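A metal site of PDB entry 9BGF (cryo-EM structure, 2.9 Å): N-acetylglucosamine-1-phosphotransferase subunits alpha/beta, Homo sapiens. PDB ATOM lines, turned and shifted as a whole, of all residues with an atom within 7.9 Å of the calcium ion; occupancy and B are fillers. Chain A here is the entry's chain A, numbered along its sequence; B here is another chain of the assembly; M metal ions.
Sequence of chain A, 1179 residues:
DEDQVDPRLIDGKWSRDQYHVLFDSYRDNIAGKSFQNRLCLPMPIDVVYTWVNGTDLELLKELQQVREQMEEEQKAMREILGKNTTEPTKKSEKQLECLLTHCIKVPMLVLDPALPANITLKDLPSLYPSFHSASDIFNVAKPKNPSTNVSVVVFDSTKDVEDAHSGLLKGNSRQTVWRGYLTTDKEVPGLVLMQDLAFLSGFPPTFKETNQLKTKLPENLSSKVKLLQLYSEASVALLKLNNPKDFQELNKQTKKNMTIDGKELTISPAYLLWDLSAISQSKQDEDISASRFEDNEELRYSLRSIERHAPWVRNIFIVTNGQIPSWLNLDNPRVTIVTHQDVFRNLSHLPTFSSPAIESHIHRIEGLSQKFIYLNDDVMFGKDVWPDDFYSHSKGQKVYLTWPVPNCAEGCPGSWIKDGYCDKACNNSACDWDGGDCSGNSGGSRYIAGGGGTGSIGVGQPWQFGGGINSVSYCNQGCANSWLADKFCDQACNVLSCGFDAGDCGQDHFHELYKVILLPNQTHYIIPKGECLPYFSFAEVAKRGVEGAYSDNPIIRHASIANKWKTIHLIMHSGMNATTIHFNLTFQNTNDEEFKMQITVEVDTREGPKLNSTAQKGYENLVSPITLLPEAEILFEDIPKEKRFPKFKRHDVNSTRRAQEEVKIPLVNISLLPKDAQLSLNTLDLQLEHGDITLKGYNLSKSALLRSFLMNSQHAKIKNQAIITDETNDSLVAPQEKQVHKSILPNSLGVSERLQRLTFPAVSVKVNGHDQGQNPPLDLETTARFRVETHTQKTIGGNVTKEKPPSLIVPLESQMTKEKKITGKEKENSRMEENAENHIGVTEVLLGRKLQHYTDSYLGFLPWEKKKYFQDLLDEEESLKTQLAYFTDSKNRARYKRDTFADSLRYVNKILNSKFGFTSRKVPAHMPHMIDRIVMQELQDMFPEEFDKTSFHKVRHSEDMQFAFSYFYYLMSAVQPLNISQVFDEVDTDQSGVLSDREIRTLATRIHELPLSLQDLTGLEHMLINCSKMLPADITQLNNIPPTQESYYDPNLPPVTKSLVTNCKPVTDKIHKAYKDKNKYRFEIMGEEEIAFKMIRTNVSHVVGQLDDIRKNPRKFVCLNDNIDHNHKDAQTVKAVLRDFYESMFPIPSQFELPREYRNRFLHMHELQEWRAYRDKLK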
ATOM      1  N   PHE A 984      -5.750   1.460 -13.986  1.00  0.00           N
ATOM      2  CA  PHE A 984      -4.696   0.634 -13.408  1.00  0.00           C
ATOM      3  C   PHE A 984      -3.815   1.463 -12.474  1.00  0.00           C
ATOM      4  O   PHE A 984      -3.460   1.003 -11.381  1.00  0.00           O
ATOM      5  CB  PHE A 984      -3.856  -0.002 -14.510  1.00  0.00           C
ATOM      6  CG  PHE A 984      -2.846  -0.986 -14.000  1.00  0.00           C
ATOM      7  CD1 PHE A 984      -3.176  -2.322 -13.832  1.00  0.00           C
ATOM      8  CD2 PHE A 984      -1.555  -0.585 -13.688  1.00  0.00           C
ATOM      9  CE1 PHE A 984      -2.254  -3.223 -13.368  1.00  0.00           C
ATOM     10  CE2 PHE A 984      -0.629  -1.493 -13.219  1.00  0.00           C
ATOM     11  CZ  PHE A 984      -0.976  -2.819 -13.060  1.00  0.00           C
ATOM     12  N   VAL A 987      -5.525   2.066  -9.273  1.00  0.00           N
ATOM     13  CA  VAL A 987      -5.640   0.858  -8.460  1.00  0.00           C
ATOM     14  C   VAL A 987      -4.280   0.402  -7.949  1.00  0.00           C
ATOM     15  O   VAL A 987      -4.157  -0.060  -6.815  1.00  0.00           O
ATOM     16  CB  VAL A 987      -6.358  -0.251  -9.261  1.00  0.00           C
ATOM     17  CG1 VAL A 987      -6.193  -1.587  -8.575  1.00  0.00           C
ATOM     18  CG2 VAL A 987      -7.832   0.085  -9.409  1.00  0.00           C
ATOM     19  N   ASP A 988      -3.240   0.521  -8.778  1.00  0.00           N
ATOM     20  CA  ASP A 988      -1.892   0.137  -8.377  1.00  0.00           C
ATOM     21  C   ASP A 988      -1.292   1.261  -7.544  1.00  0.00           C
ATOM     22  O   ASP A 988      -0.507   2.094  -8.013  1.00  0.00           O
ATOM     23  CB  ASP A 988      -1.040  -0.177  -9.599  1.00  0.00           C
ATOM     24  CG  ASP A 988       0.396  -0.515  -9.258  1.00  0.00           C
ATOM     25  OD1 ASP A 988       0.635  -1.592  -8.675  1.00  0.00           O
ATOM     26  OD2 ASP A 988       1.284   0.295  -9.573  1.00  0.00           O
ATOM     27  N   THR A 989      -1.672   1.299  -6.264  1.00  0.00           N
ATOM     28  CA  THR A 989      -1.201   2.339  -5.370  1.00  0.00           C
ATOM     29  C   THR A 989       0.270   2.178  -5.015  1.00  0.00           C
ATOM     30  O   THR A 989       0.890   3.131  -4.532  1.00  0.00           O
ATOM     31  CB  THR A 989      -2.039   2.364  -4.092  1.00  0.00           C
ATOM     32  OG1 THR A 989      -1.961   1.086  -3.445  1.00  0.00           O
ATOM     33  CG2 THR A 989      -3.493   2.641  -4.424  1.00  0.00           C
ATOM     34  N   ASP A 990       0.846   0.998  -5.248  1.00  0.00           N
ATOM     35  CA  ASP A 990       2.270   0.792  -5.014  1.00  0.00           C
ATOM     36  C   ASP A 990       3.146   1.555  -6.003  1.00  0.00           C
ATOM     37  O   ASP A 990       4.332   1.738  -5.739  1.00  0.00           O
ATOM     38  CB  ASP A 990       2.590  -0.710  -5.089  1.00  0.00           C
ATOM     39  CG  ASP A 990       3.846  -1.077  -4.333  1.00  0.00           C
ATOM     40  OD1 ASP A 990       4.059  -2.295  -4.101  1.00  0.00           O
ATOM     41  OD2 ASP A 990       4.618  -0.180  -3.938  1.00  0.00           O
ATOM     42  N   GLN A 991       2.583   1.999  -7.121  1.00  0.00           N
ATOM     43  CA  GLN A 991       3.338   2.643  -8.200  1.00  0.00           C
ATOM     44  C   GLN A 991       4.440   1.713  -8.711  1.00  0.00           C
ATOM     45  O   GLN A 991       5.531   2.144  -9.055  1.00  0.00           O
ATOM     46  CB  GLN A 991       3.915   3.978  -7.746  1.00  0.00           C
ATOM     47  CG  GLN A 991       2.883   4.989  -7.272  1.00  0.00           C
ATOM     48  CD  GLN A 991       2.159   5.668  -8.409  1.00  0.00           C
ATOM     49  OE1 GLN A 991       2.548   6.746  -8.855  1.00  0.00           O
ATOM     50  NE2 GLN A 991       1.093   5.045  -8.902  1.00  0.00           N
ATOM     51  N   SER A 992       4.127   0.420  -8.758  1.00  0.00           N
ATOM     52  CA  SER A 992       5.086  -0.594  -9.182  1.00  0.00           C
ATOM     53  C   SER A 992       4.779  -1.214 -10.528  1.00  0.00           C
ATOM     54  O   SER A 992       5.663  -1.829 -11.127  1.00  0.00           O
ATOM     55  CB  SER A 992       5.164  -1.716  -8.132  1.00  0.00           C
ATOM     56  OG  SER A 992       3.903  -2.333  -7.956  1.00  0.00           O
ATOM     57  N   GLY A 993       3.553  -1.069 -11.024  1.00  0.00           N
ATOM     58  CA  GLY A 993       3.148  -1.659 -12.283  1.00  0.00           C
ATOM     59  C   GLY A 993       2.553  -3.039 -12.183  1.00  0.00           C
ATOM     60  O   GLY A 993       2.053  -3.554 -13.185  1.00  0.00           O
ATOM     61  N   VAL A 994       2.585  -3.660 -11.002  1.00  0.00           N
ATOM     62  CA  VAL A 994       2.047  -4.998 -10.791  1.00  0.00           C
ATOM     63  C   VAL A 994       1.021  -4.933  -9.673  1.00  0.00           C
ATOM     64  O   VAL A 994       1.303  -4.375  -8.602  1.00  0.00           O
ATOM     65  CB  VAL A 994       3.155  -6.013 -10.457  1.00  0.00           C
ATOM     66  CG1 VAL A 994       2.596  -7.417 -10.427  1.00  0.00           C
ATOM     67  CG2 VAL A 994       4.303  -5.904 -11.440  1.00  0.00           C
ATOM     68  N   LEU A 995      -0.162  -5.487  -9.918  1.00  0.00           N
ATOM     69  CA  LEU A 995      -1.221  -5.500  -8.919  1.00  0.00           C
ATOM     70  C   LEU A 995      -0.937  -6.559  -7.870  1.00  0.00           C
ATOM     71  O   LEU A 995      -0.759  -7.742  -8.200  1.00  0.00           O
ATOM     72  CB  LEU A 995      -2.578  -5.749  -9.565  1.00  0.00           C
ATOM     73  CG  LEU A 995      -3.226  -4.609 -10.364  1.00  0.00           C
ATOM     74  CD1 LEU A 995      -4.681  -4.922 -10.627  1.00  0.00           C
ATOM     75  CD2 LEU A 995      -3.072  -3.283  -9.641  1.00  0.00           C
ATOM     76  N   SER A 996      -0.900  -6.150  -6.600  1.00  0.00           N
ATOM     77  CA  SER A 996      -0.811  -7.088  -5.493  1.00  0.00           C
ATOM     78  C   SER A 996      -2.191  -7.644  -5.179  1.00  0.00           C
ATOM     79  O   SER A 996      -3.201  -7.267  -5.774  1.00  0.00           O
ATOM     80  CB  SER A 996      -0.215  -6.412  -4.268  1.00  0.00           C
ATOM     81  OG  SER A 996       1.052  -5.837  -4.565  1.00  0.00           O
ATOM     82  N   ASP A 997      -2.241  -8.578  -4.224  1.00  0.00           N
ATOM     83  CA  ASP A 997      -3.513  -9.180  -3.854  1.00  0.00           C
ATOM     84  C   ASP A 997      -4.487  -8.135  -3.314  1.00  0.00           C
ATOM     85  O   ASP A 997      -5.682  -8.161  -3.642  1.00  0.00           O
ATOM     86  CB  ASP A 997      -3.291 -10.276  -2.805  1.00  0.00           C
ATOM     87  CG  ASP A 997      -2.268 -11.308  -3.263  1.00  0.00           C
ATOM     88  OD1 ASP A 997      -1.073 -10.964  -3.323  1.00  0.00           O
ATOM     89  OD2 ASP A 997      -2.680 -12.444  -3.547  1.00  0.00           O
ATOM     90  N   ARG A 998      -3.989  -7.211  -2.490  1.00  0.00           N
ATOM     91  CA  ARG A 998      -4.835  -6.123  -1.990  1.00  0.00           C
ATOM     92  C   ARG A 998      -5.312  -5.231  -3.133  1.00  0.00           C
ATOM     93  O   ARG A 998      -6.483  -4.830  -3.163  1.00  0.00           O
ATOM     94  CB  ARG A 998      -4.059  -5.323  -0.948  1.00  0.00           C
ATOM     95  CG  ARG A 998      -2.701  -4.855  -1.436  1.00  0.00           C
ATOM     96  CD  ARG A 998      -1.836  -4.345  -0.306  1.00  0.00           C
ATOM     97  NE  ARG A 998      -1.589  -5.359   0.703  1.00  0.00           N
ATOM     98  CZ  ARG A 998      -0.528  -5.391   1.498  1.00  0.00           C
ATOM     99  NH1 ARG A 998       0.429  -4.474   1.396  1.00  0.00           N
ATOM    100  NH2 ARG A 998      -0.428  -6.350   2.403  1.00  0.00           N
ATOM    101  N   GLU A 999      -4.430  -4.917  -4.078  1.00  0.00           N
ATOM    102  CA  GLU A 999      -4.813  -4.085  -5.205  1.00  0.00           C
ATOM    103  C   GLU A 999      -5.770  -4.827  -6.137  1.00  0.00           C
ATOM    104  O   GLU A 999      -6.683  -4.219  -6.697  1.00  0.00           O
ATOM    105  CB  GLU A 999      -3.561  -3.626  -5.951  1.00  0.00           C
ATOM    106  CG  GLU A 999      -2.594  -2.892  -5.037  1.00  0.00           C
ATOM    107  CD  GLU A 999      -1.288  -2.536  -5.722  1.00  0.00           C
ATOM    108  OE1 GLU A 999      -1.077  -2.968  -6.870  1.00  0.00           O
ATOM    109  OE2 GLU A 999      -0.475  -1.823  -5.096  1.00  0.00           O
ATOM    110  N   ILE A1000      -5.585  -6.138  -6.284  1.00  0.00           N
ATOM    111  CA  ILE A1000      -6.537  -6.932  -7.058  1.00  0.00           C
ATOM    112  C   ILE A1000      -7.905  -6.930  -6.384  1.00  0.00           C
ATOM    113  O   ILE A1000      -8.942  -6.884  -7.061  1.00  0.00           O
ATOM    114  CB  ILE A1000      -6.003  -8.363  -7.268  1.00  0.00           C
ATOM    115  CG1 ILE A1000      -4.799  -8.346  -8.212  1.00  0.00           C
ATOM    116  CG2 ILE A1000      -7.083  -9.265  -7.844  1.00  0.00           C
ATOM    117  CD1 ILE A1000      -4.194  -9.707  -8.424  1.00  0.00           C
ATOM    118  N   TYR A1048       1.191 -14.221  -4.726  1.00  0.00           N
ATOM    119  CA  TYR A1048      -0.266 -14.253  -4.793  1.00  0.00           C
ATOM    120  C   TYR A1048      -0.816 -15.459  -4.045  1.00  0.00           C
ATOM    121  O   TYR A1048      -0.099 -16.429  -3.756  1.00  0.00           O
ATOM    122  CB  TYR A1048      -0.731 -14.270  -6.252  1.00  0.00           C
ATOM    123  CG  TYR A1048      -0.377 -13.024  -7.018  1.00  0.00           C
ATOM    124  CD1 TYR A1048      -1.225 -11.933  -7.038  1.00  0.00           C
ATOM    125  CD2 TYR A1048       0.827 -12.928  -7.716  1.00  0.00           C
ATOM    126  CE1 TYR A1048      -0.902 -10.789  -7.734  1.00  0.00           C
ATOM    127  CE2 TYR A1048       1.151 -11.791  -8.420  1.00  0.00           C
ATOM    128  CZ  TYR A1048       0.283 -10.724  -8.421  1.00  0.00           C
ATOM    129  OH  TYR A1048       0.597  -9.584  -9.115  1.00  0.00           O
ATOM    130  N   VAL A1056       0.269  -9.556 -12.296  1.00  0.00           N
ATOM    131  CA  VAL A1056      -0.761  -8.794 -13.001  1.00  0.00           C
ATOM    132  C   VAL A1056      -0.189  -7.440 -13.403  1.00  0.00           C
ATOM    133  O   VAL A1056      -0.262  -6.471 -12.635  1.00  0.00           O
ATOM    134  CB  VAL A1056      -2.014  -8.638 -12.124  1.00  0.00           C
ATOM    135  CG1 VAL A1056      -3.095  -7.894 -12.881  1.00  0.00           C
ATOM    136  CG2 VAL A1056      -2.520 -10.003 -11.696  1.00  0.00           C
ATOM    137  N   PRO B1147       0.480   2.423   0.521  1.00  0.00           N
ATOM    138  CA  PRO B1147       1.620   1.534   0.779  1.00  0.00           C
ATOM    139  C   PRO B1147       2.958   2.234   0.901  1.00  0.00           C
ATOM    140  O   PRO B1147       3.871   1.669   1.529  1.00  0.00           O
ATOM    141  CB  PRO B1147       1.606   0.606  -0.440  1.00  0.00           C
ATOM    142  CG  PRO B1147       1.068   1.462  -1.531  1.00  0.00           C
ATOM    143  CD  PRO B1147       0.066   2.393  -0.886  1.00  0.00           C
HETATM  144 CA    CA M   1       1.344  -2.781  -6.890  1.00  0.00          CA
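The backbone NH (N) of Gly 993 is in hydrogen-bond range of the side-chain carboxylate (OD2) of Asp 988 (3.0 Å).
The side-chain carboxylate (OE1) of Glu 999 lies close to the backbone NH (N) of Ser 996, at 3.2 Å.
The backbone NH (N) of Gln 991 sits at hydrogen-bond distance from the side-chain carboxylate (OD2) of Asp 988 (3.3 Å).
The backbone NH of Asp 990 lies close to the side-chain carboxylate of Glu 999 (3.1 Å).
CB of Asp 990 touches the calcium ion, at 3.0 Å.
Ser 996 touches the calcium ion (OG to CA, 3.9 Å).
The nearest printed residue that does not touch the calcium ion is Leu 995 (4.3 Å).
The calcium ion is bound by OD1 of Asp 988 (2.3 Å), O of Val 994 (2.3 Å), OE1 of Glu 999 (2.4 Å), OE2 of Glu 999 (2.7 Å) and OG of Ser 992 (2.8 Å).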
